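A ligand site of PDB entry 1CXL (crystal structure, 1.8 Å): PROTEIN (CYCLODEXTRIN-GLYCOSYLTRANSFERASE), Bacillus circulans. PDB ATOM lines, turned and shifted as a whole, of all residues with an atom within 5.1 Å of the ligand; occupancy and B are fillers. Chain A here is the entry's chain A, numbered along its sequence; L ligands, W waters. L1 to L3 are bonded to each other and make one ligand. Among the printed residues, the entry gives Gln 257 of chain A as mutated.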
ATOM      1  N   PHE A  21      14.758  33.211  25.636  1.00  0.00           N
ATOM      2  CA  PHE A  21      16.132  33.663  25.807  1.00  0.00           C
ATOM      3  C   PHE A  21      15.957  34.667  26.906  1.00  0.00           C
ATOM      4  O   PHE A  21      15.531  35.785  26.667  1.00  0.00           O
ATOM      5  CB  PHE A  21      16.722  34.342  24.555  1.00  0.00           C
ATOM      6  CG  PHE A  21      18.043  33.753  24.135  1.00  0.00           C
ATOM      7  CD1 PHE A  21      18.115  32.467  23.606  1.00  0.00           C
ATOM      8  CD2 PHE A  21      19.224  34.478  24.277  1.00  0.00           C
ATOM      9  CE1 PHE A  21      19.329  31.906  23.205  1.00  0.00           C
ATOM     10  CE2 PHE A  21      20.455  33.942  23.879  1.00  0.00           C
ATOM     11  CZ  PHE A  21      20.497  32.652  23.346  1.00  0.00           C
ATOM     12  N   ARG A  47      25.350  41.485  21.938  1.00  0.00           N
ATOM     13  CA  ARG A  47      26.280  40.571  22.589  1.00  0.00           C
ATOM     14  C   ARG A  47      26.452  40.881  24.072  1.00  0.00           C
ATOM     15  O   ARG A  47      27.174  40.193  24.783  1.00  0.00           O
ATOM     16  CB  ARG A  47      27.619  40.512  21.889  1.00  0.00           C
ATOM     17  CG  ARG A  47      27.551  39.810  20.549  1.00  0.00           C
ATOM     18  CD  ARG A  47      28.895  39.787  19.846  1.00  0.00           C
ATOM     19  NE  ARG A  47      28.780  39.638  18.403  1.00  0.00           N
ATOM     20  CZ  ARG A  47      28.828  38.462  17.782  1.00  0.00           C
ATOM     21  NH1 ARG A  47      28.982  37.325  18.458  1.00  0.00           N
ATOM     22  NH2 ARG A  47      28.717  38.413  16.459  1.00  0.00           N
ATOM     23  N   ASN A  94      31.899  40.630  24.273  1.00  0.00           N
ATOM     24  CA  ASN A  94      30.961  39.535  24.438  1.00  0.00           C
ATOM     25  C   ASN A  94      30.749  39.192  25.904  1.00  0.00           C
ATOM     26  O   ASN A  94      31.687  39.213  26.708  1.00  0.00           O
ATOM     27  CB  ASN A  94      31.432  38.258  23.699  1.00  0.00           C
ATOM     28  CG  ASN A  94      31.254  38.340  22.202  1.00  0.00           C
ATOM     29  OD1 ASN A  94      30.282  37.793  21.646  1.00  0.00           O
ATOM     30  ND2 ASN A  94      32.181  39.013  21.540  1.00  0.00           N
ATOM     31  N   TYR A  97      25.387  36.608  28.431  1.00  0.00           N
ATOM     32  CA  TYR A  97      23.946  36.833  28.446  1.00  0.00           C
ATOM     33  C   TYR A  97      23.158  35.602  28.010  1.00  0.00           C
ATOM     34  O   TYR A  97      22.027  35.399  28.430  1.00  0.00           O
ATOM     35  CB  TYR A  97      23.558  38.013  27.554  1.00  0.00           C
ATOM     36  CG  TYR A  97      23.628  37.603  26.112  1.00  0.00           C
ATOM     37  CD1 TYR A  97      24.838  37.658  25.430  1.00  0.00           C
ATOM     38  CD2 TYR A  97      22.510  37.119  25.444  1.00  0.00           C
ATOM     39  CE1 TYR A  97      24.933  37.261  24.108  1.00  0.00           C
ATOM     40  CE2 TYR A  97      22.577  36.714  24.106  1.00  0.00           C
ATOM     41  CZ  TYR A  97      23.793  36.783  23.442  1.00  0.00           C
ATOM     42  OH  TYR A  97      23.884  36.399  22.138  1.00  0.00           O
ATOM     43  N   HIS A  98      23.756  34.796  27.147  1.00  0.00           N
ATOM     44  CA  HIS A  98      23.116  33.606  26.617  1.00  0.00           C
ATOM     45  C   HIS A  98      22.978  32.460  27.632  1.00  0.00           C
ATOM     46  O   HIS A  98      22.171  31.543  27.446  1.00  0.00           O
ATOM     47  CB  HIS A  98      23.797  33.124  25.317  1.00  0.00           C
ATOM     48  CG  HIS A  98      25.271  33.052  25.462  1.00  0.00           C
ATOM     49  ND1 HIS A  98      25.877  32.089  26.250  1.00  0.00           N
ATOM     50  CD2 HIS A  98      26.248  33.854  24.923  1.00  0.00           C
ATOM     51  CE1 HIS A  98      27.190  32.294  26.167  1.00  0.00           C
ATOM     52  NE2 HIS A  98      27.445  33.347  25.381  1.00  0.00           N
ATOM     53  N   TYR A 100      25.248  30.137  28.400  1.00  0.00           N
ATOM     54  CA  TYR A 100      25.971  28.897  28.065  1.00  0.00           C
ATOM     55  C   TYR A 100      27.406  28.766  28.514  1.00  0.00           C
ATOM     56  O   TYR A 100      28.064  27.793  28.188  1.00  0.00           O
ATOM     57  CB  TYR A 100      25.870  28.533  26.558  1.00  0.00           C
ATOM     58  CG  TYR A 100      24.463  28.202  26.111  1.00  0.00           C
ATOM     59  CD1 TYR A 100      23.868  26.984  26.423  1.00  0.00           C
ATOM     60  CD2 TYR A 100      23.736  29.128  25.352  1.00  0.00           C
ATOM     61  CE1 TYR A 100      22.578  26.677  25.994  1.00  0.00           C
ATOM     62  CE2 TYR A 100      22.442  28.843  24.923  1.00  0.00           C
ATOM     63  CZ  TYR A 100      21.869  27.614  25.242  1.00  0.00           C
ATOM     64  OH  TYR A 100      20.606  27.342  24.799  1.00  0.00           O
ATOM     65  N   TRP A 101      27.894  29.753  29.259  1.00  0.00           N
ATOM     66  CA  TRP A 101      29.257  29.740  29.764  1.00  0.00           C
ATOM     67  C   TRP A 101      29.248  29.590  31.283  1.00  0.00           C
ATOM     68  O   TRP A 101      29.468  30.548  32.009  1.00  0.00           O
ATOM     69  CB  TRP A 101      29.967  31.054  29.395  1.00  0.00           C
ATOM     70  CG  TRP A 101      30.146  31.258  27.923  1.00  0.00           C
ATOM     71  CD1 TRP A 101      30.065  30.312  26.952  1.00  0.00           C
ATOM     72  CD2 TRP A 101      30.456  32.484  27.262  1.00  0.00           C
ATOM     73  NE1 TRP A 101      30.303  30.870  25.721  1.00  0.00           N
ATOM     74  CE2 TRP A 101      30.533  32.202  25.886  1.00  0.00           C
ATOM     75  CE3 TRP A 101      30.665  33.792  27.717  1.00  0.00           C
ATOM     76  CZ2 TRP A 101      30.842  33.198  24.961  1.00  0.00           C
ATOM     77  CZ3 TRP A 101      30.955  34.772  26.794  1.00  0.00           C
ATOM     78  CH2 TRP A 101      31.050  34.483  25.437  1.00  0.00           C
ATOM     79  N   HIS A 140      30.659  21.652  28.890  1.00  0.00           N
ATOM     80  CA  HIS A 140      31.789  22.542  29.114  1.00  0.00           C
ATOM     81  C   HIS A 140      31.492  23.644  30.110  1.00  0.00           C
ATOM     82  O   HIS A 140      30.371  23.820  30.566  1.00  0.00           O
ATOM     83  CB  HIS A 140      32.072  23.259  27.764  1.00  0.00           C
ATOM     84  CG  HIS A 140      30.812  23.871  27.210  1.00  0.00           C
ATOM     85  ND1 HIS A 140      30.013  23.192  26.280  1.00  0.00           N
ATOM     86  CD2 HIS A 140      30.215  25.068  27.474  1.00  0.00           C
ATOM     87  CE1 HIS A 140      28.983  23.981  25.998  1.00  0.00           C
ATOM     88  NE2 HIS A 140      29.062  25.115  26.705  1.00  0.00           N
ATOM     89  N   PRO A 143      34.853  29.886  27.848  1.00  0.00           N
ATOM     90  CA  PRO A 143      36.012  30.110  26.991  1.00  0.00           C
ATOM     91  C   PRO A 143      37.309  30.112  27.782  1.00  0.00           C
ATOM     92  O   PRO A 143      37.431  30.752  28.812  1.00  0.00           O
ATOM     93  CB  PRO A 143      35.785  31.450  26.292  1.00  0.00           C
ATOM     94  CG  PRO A 143      34.307  31.756  26.447  1.00  0.00           C
ATOM     95  CD  PRO A 143      33.801  30.903  27.602  1.00  0.00           C
ATOM     96  N   LEU A 194      34.879  22.419  21.989  1.00  0.00           N
ATOM     97  CA  LEU A 194      33.984  23.071  21.060  1.00  0.00           C
ATOM     98  C   LEU A 194      34.502  24.479  21.020  1.00  0.00           C
ATOM     99  O   LEU A 194      34.397  25.203  22.002  1.00  0.00           O
ATOM    100  CB  LEU A 194      32.547  23.163  21.613  1.00  0.00           C
ATOM    101  CG  LEU A 194      31.683  21.945  21.372  1.00  0.00           C
ATOM    102  CD1 LEU A 194      30.329  22.188  22.018  1.00  0.00           C
ATOM    103  CD2 LEU A 194      31.512  21.735  19.872  1.00  0.00           C
ATOM    104  N   TYR A 195      35.119  24.877  19.930  1.00  0.00           N
ATOM    105  CA  TYR A 195      35.665  26.217  19.902  1.00  0.00           C
ATOM    106  C   TYR A 195      36.728  26.352  20.973  1.00  0.00           C
ATOM    107  O   TYR A 195      37.656  25.549  21.018  1.00  0.00           O
ATOM    108  CB  TYR A 195      34.552  27.263  20.050  1.00  0.00           C
ATOM    109  CG  TYR A 195      33.437  26.932  19.101  1.00  0.00           C
ATOM    110  CD1 TYR A 195      33.736  26.610  17.772  1.00  0.00           C
ATOM    111  CD2 TYR A 195      32.096  26.891  19.502  1.00  0.00           C
ATOM    112  CE1 TYR A 195      32.740  26.271  16.860  1.00  0.00           C
ATOM    113  CE2 TYR A 195      31.086  26.564  18.606  1.00  0.00           C
ATOM    114  CZ  TYR A 195      31.413  26.254  17.285  1.00  0.00           C
ATOM    115  OH  TYR A 195      30.423  25.930  16.391  1.00  0.00           O
ATOM    116  N   ASP A 196      36.593  27.347  21.834  1.00  0.00           N
ATOM    117  CA  ASP A 196      37.557  27.556  22.904  1.00  0.00           C
ATOM    118  C   ASP A 196      36.950  27.232  24.256  1.00  0.00           C
ATOM    119  O   ASP A 196      37.454  27.672  25.284  1.00  0.00           O
ATOM    120  CB  ASP A 196      38.019  29.025  22.926  1.00  0.00           C
ATOM    121  CG  ASP A 196      36.853  29.966  23.039  1.00  0.00           C
ATOM    122  OD1 ASP A 196      35.713  29.584  23.131  1.00  0.00           O
ATOM    123  OD2 ASP A 196      37.208  31.218  23.001  1.00  0.00           O
ATOM    124  N   LEU A 197      35.848  26.494  24.236  1.00  0.00           N
ATOM    125  CA  LEU A 197      35.159  26.136  25.466  1.00  0.00           C
ATOM    126  C   LEU A 197      35.852  25.013  26.200  1.00  0.00           C
ATOM    127  O   LEU A 197      36.074  23.944  25.632  1.00  0.00           O
ATOM    128  CB  LEU A 197      33.668  25.787  25.229  1.00  0.00           C
ATOM    129  CG  LEU A 197      32.867  26.879  24.496  1.00  0.00           C
ATOM    130  CD1 LEU A 197      31.521  26.304  24.039  1.00  0.00           C
ATOM    131  CD2 LEU A 197      32.638  28.079  25.411  1.00  0.00           C
ATOM    132  N   ARG A 227      16.616  20.562  28.922  1.00  0.00           N
ATOM    133  CA  ARG A 227      17.082  20.644  27.550  1.00  0.00           C
ATOM    134  C   ARG A 227      18.600  20.523  27.626  1.00  0.00           C
ATOM    135  O   ARG A 227      19.258  21.427  28.146  1.00  0.00           O
ATOM    136  CB  ARG A 227      16.664  21.919  26.818  1.00  0.00           C
ATOM    137  CG  ARG A 227      17.156  21.954  25.367  1.00  0.00           C
ATOM    138  CD  ARG A 227      18.588  22.485  25.221  1.00  0.00           C
ATOM    139  NE  ARG A 227      18.882  22.959  23.861  1.00  0.00           N
ATOM    140  CZ  ARG A 227      20.005  23.613  23.536  1.00  0.00           C
ATOM    141  NH1 ARG A 227      20.960  23.902  24.421  1.00  0.00           N
ATOM    142  NH2 ARG A 227      20.158  23.994  22.266  1.00  0.00           N
ATOM    143  N   ASP A 229      22.252  20.625  26.325  1.00  0.00           N
ATOM    144  CA  ASP A 229      23.051  21.227  25.282  1.00  0.00           C
ATOM    145  C   ASP A 229      24.197  20.323  24.792  1.00  0.00           C
ATOM    146  O   ASP A 229      24.847  19.654  25.576  1.00  0.00           O
ATOM    147  CB  ASP A 229      23.618  22.561  25.769  1.00  0.00           C
ATOM    148  CG  ASP A 229      24.494  23.241  24.758  1.00  0.00           C
ATOM    149  OD1 ASP A 229      25.660  22.827  24.610  1.00  0.00           O
ATOM    150  OD2 ASP A 229      23.986  24.212  24.080  1.00  0.00           O
ATOM    151  N   ALA A 230      24.422  20.335  23.472  1.00  0.00           N
ATOM    152  CA  ALA A 230      25.534  19.602  22.832  1.00  0.00           C
ATOM    153  C   ALA A 230      25.662  18.118  23.149  1.00  0.00           C
ATOM    154  O   ALA A 230      26.757  17.657  23.479  1.00  0.00           O
ATOM    155  CB  ALA A 230      26.822  20.314  23.198  1.00  0.00           C
ATOM    156  N   GLN A 257      20.225  18.441  22.446  1.00  0.00           N
ATOM    157  CA  GLN A 257      20.528  19.179  21.243  1.00  0.00           C
ATOM    158  C   GLN A 257      21.623  18.471  20.457  1.00  0.00           C
ATOM    159  O   GLN A 257      22.778  18.418  20.875  1.00  0.00           O
ATOM    160  CB  GLN A 257      20.948  20.620  21.575  1.00  0.00           C
ATOM    161  CG  GLN A 257      21.458  21.357  20.338  1.00  0.00           C
ATOM    162  CD  GLN A 257      22.654  22.224  20.632  1.00  0.00           C
ATOM    163  OE1 GLN A 257      23.376  22.011  21.618  1.00  0.00           O
ATOM    164  NE2 GLN A 257      22.863  23.226  19.772  1.00  0.00           N
ATOM    165  N   HIS A 327      17.869  29.723  18.560  1.00  0.00           N
ATOM    166  CA  HIS A 327      18.901  30.737  18.796  1.00  0.00           C
ATOM    167  C   HIS A 327      20.234  30.464  18.111  1.00  0.00           C
ATOM    168  O   HIS A 327      21.158  31.274  18.192  1.00  0.00           O
ATOM    169  CB  HIS A 327      19.128  30.891  20.315  1.00  0.00           C
ATOM    170  CG  HIS A 327      19.642  29.604  20.855  1.00  0.00           C
ATOM    171  ND1 HIS A 327      18.846  28.477  20.888  1.00  0.00           N
ATOM    172  CD2 HIS A 327      20.865  29.272  21.336  1.00  0.00           C
ATOM    173  CE1 HIS A 327      19.580  27.489  21.389  1.00  0.00           C
ATOM    174  NE2 HIS A 327      20.810  27.936  21.673  1.00  0.00           N
ATOM    175  N   ASP A 328      20.335  29.321  17.442  1.00  0.00           N
ATOM    176  CA  ASP A 328      21.551  28.927  16.756  1.00  0.00           C
ATOM    177  C   ASP A 328      21.380  28.879  15.249  1.00  0.00           C
ATOM    178  O   ASP A 328      22.222  28.338  14.535  1.00  0.00           O
ATOM    179  CB  ASP A 328      22.101  27.591  17.295  1.00  0.00           C
ATOM    180  CG  ASP A 328      22.590  27.692  18.722  1.00  0.00           C
ATOM    181  OD1 ASP A 328      23.111  28.673  19.195  1.00  0.00           O
ATOM    182  OD2 ASP A 328      22.396  26.583  19.393  1.00  0.00           O
ATOM    183  N   ASP A 371      23.500  34.254  14.872  1.00  0.00           N
ATOM    184  CA  ASP A 371      23.892  34.748  16.180  1.00  0.00           C
ATOM    185  C   ASP A 371      24.856  35.936  16.041  1.00  0.00           C
ATOM    186  O   ASP A 371      25.825  35.862  15.302  1.00  0.00           O
ATOM    187  CB  ASP A 371      24.564  33.572  16.897  1.00  0.00           C
ATOM    188  CG  ASP A 371      25.305  33.939  18.137  1.00  0.00           C
ATOM    189  OD1 ASP A 371      25.092  34.950  18.777  1.00  0.00           O
ATOM    190  OD2 ASP A 371      26.180  33.035  18.476  1.00  0.00           O
ATOM    191  N   ARG A 375      18.755  36.896  18.213  1.00  0.00           N
ATOM    192  CA  ARG A 375      18.487  37.037  19.643  1.00  0.00           C
ATOM    193  C   ARG A 375      18.104  38.451  20.097  1.00  0.00           C
ATOM    194  O   ARG A 375      18.479  38.879  21.190  1.00  0.00           O
ATOM    195  CB  ARG A 375      19.651  36.518  20.475  1.00  0.00           C
ATOM    196  CG  ARG A 375      20.058  35.094  20.095  1.00  0.00           C
ATOM    197  CD  ARG A 375      21.551  34.827  20.276  1.00  0.00           C
ATOM    198  NE  ARG A 375      21.946  33.460  19.936  1.00  0.00           N
ATOM    199  CZ  ARG A 375      22.972  32.833  20.503  1.00  0.00           C
ATOM    200  NH1 ARG A 375      23.721  33.420  21.440  1.00  0.00           N
ATOM    201  NH2 ARG A 375      23.265  31.579  20.126  1.00  0.00           N
HETATM  202  C1  LIG L   1      24.730  24.874  23.009  1.00  0.00           C
HETATM  203  C2  LIG L   1      23.850  26.061  22.668  1.00  0.00           C
HETATM  204  C3  LIG L   1      24.611  27.110  21.896  1.00  0.00           C
HETATM  205  C4  LIG L   1      25.866  27.450  22.677  1.00  0.00           C
HETATM  206  C5  LIG L   1      26.713  26.204  22.761  1.00  0.00           C
HETATM  207  C6  LIG L   1      28.078  26.403  23.364  1.00  0.00           C
HETATM  208  O1  LIG L   1      22.714  25.620  21.931  1.00  0.00           O
HETATM  209  O2  LIG L   1      23.838  28.307  21.757  1.00  0.00           O
HETATM  210  O3  LIG L   1      26.563  28.540  22.069  1.00  0.00           O
HETATM  211  O4  LIG L   1      25.981  25.285  23.578  1.00  0.00           O
HETATM  212  O5  LIG L   1      28.030  27.211  24.539  1.00  0.00           O
HETATM  213  C1  LG2 L   2      27.034  29.539  22.942  1.00  0.00           C
HETATM  214  C2  LG2 L   2      26.439  30.869  22.532  1.00  0.00           C
HETATM  215  C3  LG2 L   2      27.098  31.404  21.278  1.00  0.00           C
HETATM  216  C4  LG2 L   2      28.612  31.364  21.396  1.00  0.00           C
HETATM  217  C5  LG2 L   2      29.062  29.961  21.738  1.00  0.00           C
HETATM  218  C6  LG2 L   2      30.546  29.854  21.910  1.00  0.00           C
HETATM  219  O1  LG2 L   2      25.037  30.748  22.327  1.00  0.00           O
HETATM  220  O2  LG2 L   2      26.697  32.764  21.086  1.00  0.00           O
HETATM  221  O3  LG2 L   2      29.175  31.724  20.115  1.00  0.00           O
HETATM  222  O4  LG2 L   2      28.450  29.549  22.968  1.00  0.00           O
HETATM  223  O5  LG2 L   2      30.977  30.587  23.072  1.00  0.00           O
HETATM  224  C1  LG3 L   3      30.359  32.498  20.092  1.00  0.00           C
HETATM  225  C2  LG3 L   3      30.088  33.765  19.319  1.00  0.00           C
HETATM  226  C3  LG3 L   3      29.750  33.444  17.889  1.00  0.00           C
HETATM  227  C4  LG3 L   3      30.703  32.453  17.231  1.00  0.00           C
HETATM  228  C5  LG3 L   3      31.064  31.301  18.147  1.00  0.00           C
HETATM  229  C6  LG3 L   3      32.227  30.513  17.638  1.00  0.00           C
HETATM  230  O1  LG3 L   3      29.016  34.448  19.936  1.00  0.00           O
HETATM  231  O2  LG3 L   3      29.727  34.624  17.085  1.00  0.00           O
HETATM  232  O3  LG3 L   3      31.406  31.785  19.458  1.00  0.00           O
HETATM  233  O4  LG3 L   3      32.806  31.123  16.475  1.00  0.00           O
HETATM  234  O   HOH W   1      33.574  31.132  22.581  1.00  0.00           O
HETATM  235  O   HOH W   2      26.237  36.262  20.835  1.00  0.00           O
HETATM  236  O   HOH W   3      28.569  35.022  22.678  1.00  0.00           O
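The side-chain carboxylate (OD2) of Asp 229 is covalently linked to a carbon (C1) of LIG L1.
O1 of LIG L1 is in hydrogen-bond range of NH2 of Arg 227 (3.0 Å).
An oxygen (O1) of LIG L1 is in hydrogen-bond range of a ring nitrogen (NE2) of His 327.
OD1 of Asp 328 lies within hydrogen-bond range of O2 of LIG L1 (2.7 Å).
The guanidinium group (NH1) of Arg 47 is in hydrogen-bond range of an oxygen (O2) of LG3 L3, 3.1 Å away.
NE2 of His 140 lies within hydrogen-bond range of O5 of LIG L1.
The guanidinium group (NH2) of Arg 375 sits at hydrogen-bond distance from an oxygen (O1) of LG2 L2, at 2.9 Å.
The indole nitrogen (NE1) of Trp 101 is in hydrogen-bond range of an oxygen (O5) of LG2 L2, at 2.7 Å.
OD2 of Asp 371 is in hydrogen-bond range of O2 of LG2 L2, at 2.7 Å.
The side-chain amide nitrogen (NE2) of Gln 257 is in hydrogen-bond range of an oxygen (O1) of LIG L1 (3.2 Å).
The guanidinium group of Arg 47 sits close to the side-chain amide oxygen of Asn 94.
The side-chain carboxylate (OD2) of Asp 229 lies close to the side-chain amide oxygen (OE1) of Gln 257.
OD2 of Asp 328 lies within hydrogen-bond range of NE2 of Gln 257, at 3.4 Å.
The backbone carbonyl oxygen (O) of Tyr 100 is in hydrogen-bond range of a ring nitrogen (NE2) of His 140 (3.2 Å).
The side-chain carboxylate (OD2) of Asp 328 lies within hydrogen-bond range of a ring nitrogen (NE2) of His 327.
The side-chain carboxylate of Asp 371 lies within salt-bridge range of the guanidinium group of Arg 375 (3.4 Å).
NH1 of Arg 375 lies within hydrogen-bond range of OH of Tyr 97 (3.1 Å).
N of Tyr 100 sits at hydrogen-bond distance from ND1 of His 98 (3.0 Å).
OD1 of Asn 94 touches O1 of LG3 L3, 3.96 Å away.
His 98 touches the ligand.
Tyr 100 touches the ligand.
Leu 197 touches the ligand.
Hydrophobic or aromatic side chains that line the ligand: His 98, Tyr 100, Trp 101, His 140, Leu 197 and His 327.
The nearest printed residue that does not touch the ligand is Tyr 195 (4.1 Å).
Water W1 lies within hydrogen-bond range of OD1 of Asp 196 (2.7 Å) and O5 of LG2 L2 (2.7 Å).
Water W3 lies within hydrogen-bond range of an oxygen (O1) of LG3 L3 (2.8 Å), a ring nitrogen (NE2) of His 98 (3.4 Å) and the side-chain amide oxygen of Asn 94 (3.4 Å).
Water W2 lies within hydrogen-bond range of OH of Tyr 97 (2.7 Å), OD1 of Asp 371 (2.7 Å) and O1 of LG3 L3 (3.4 Å).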
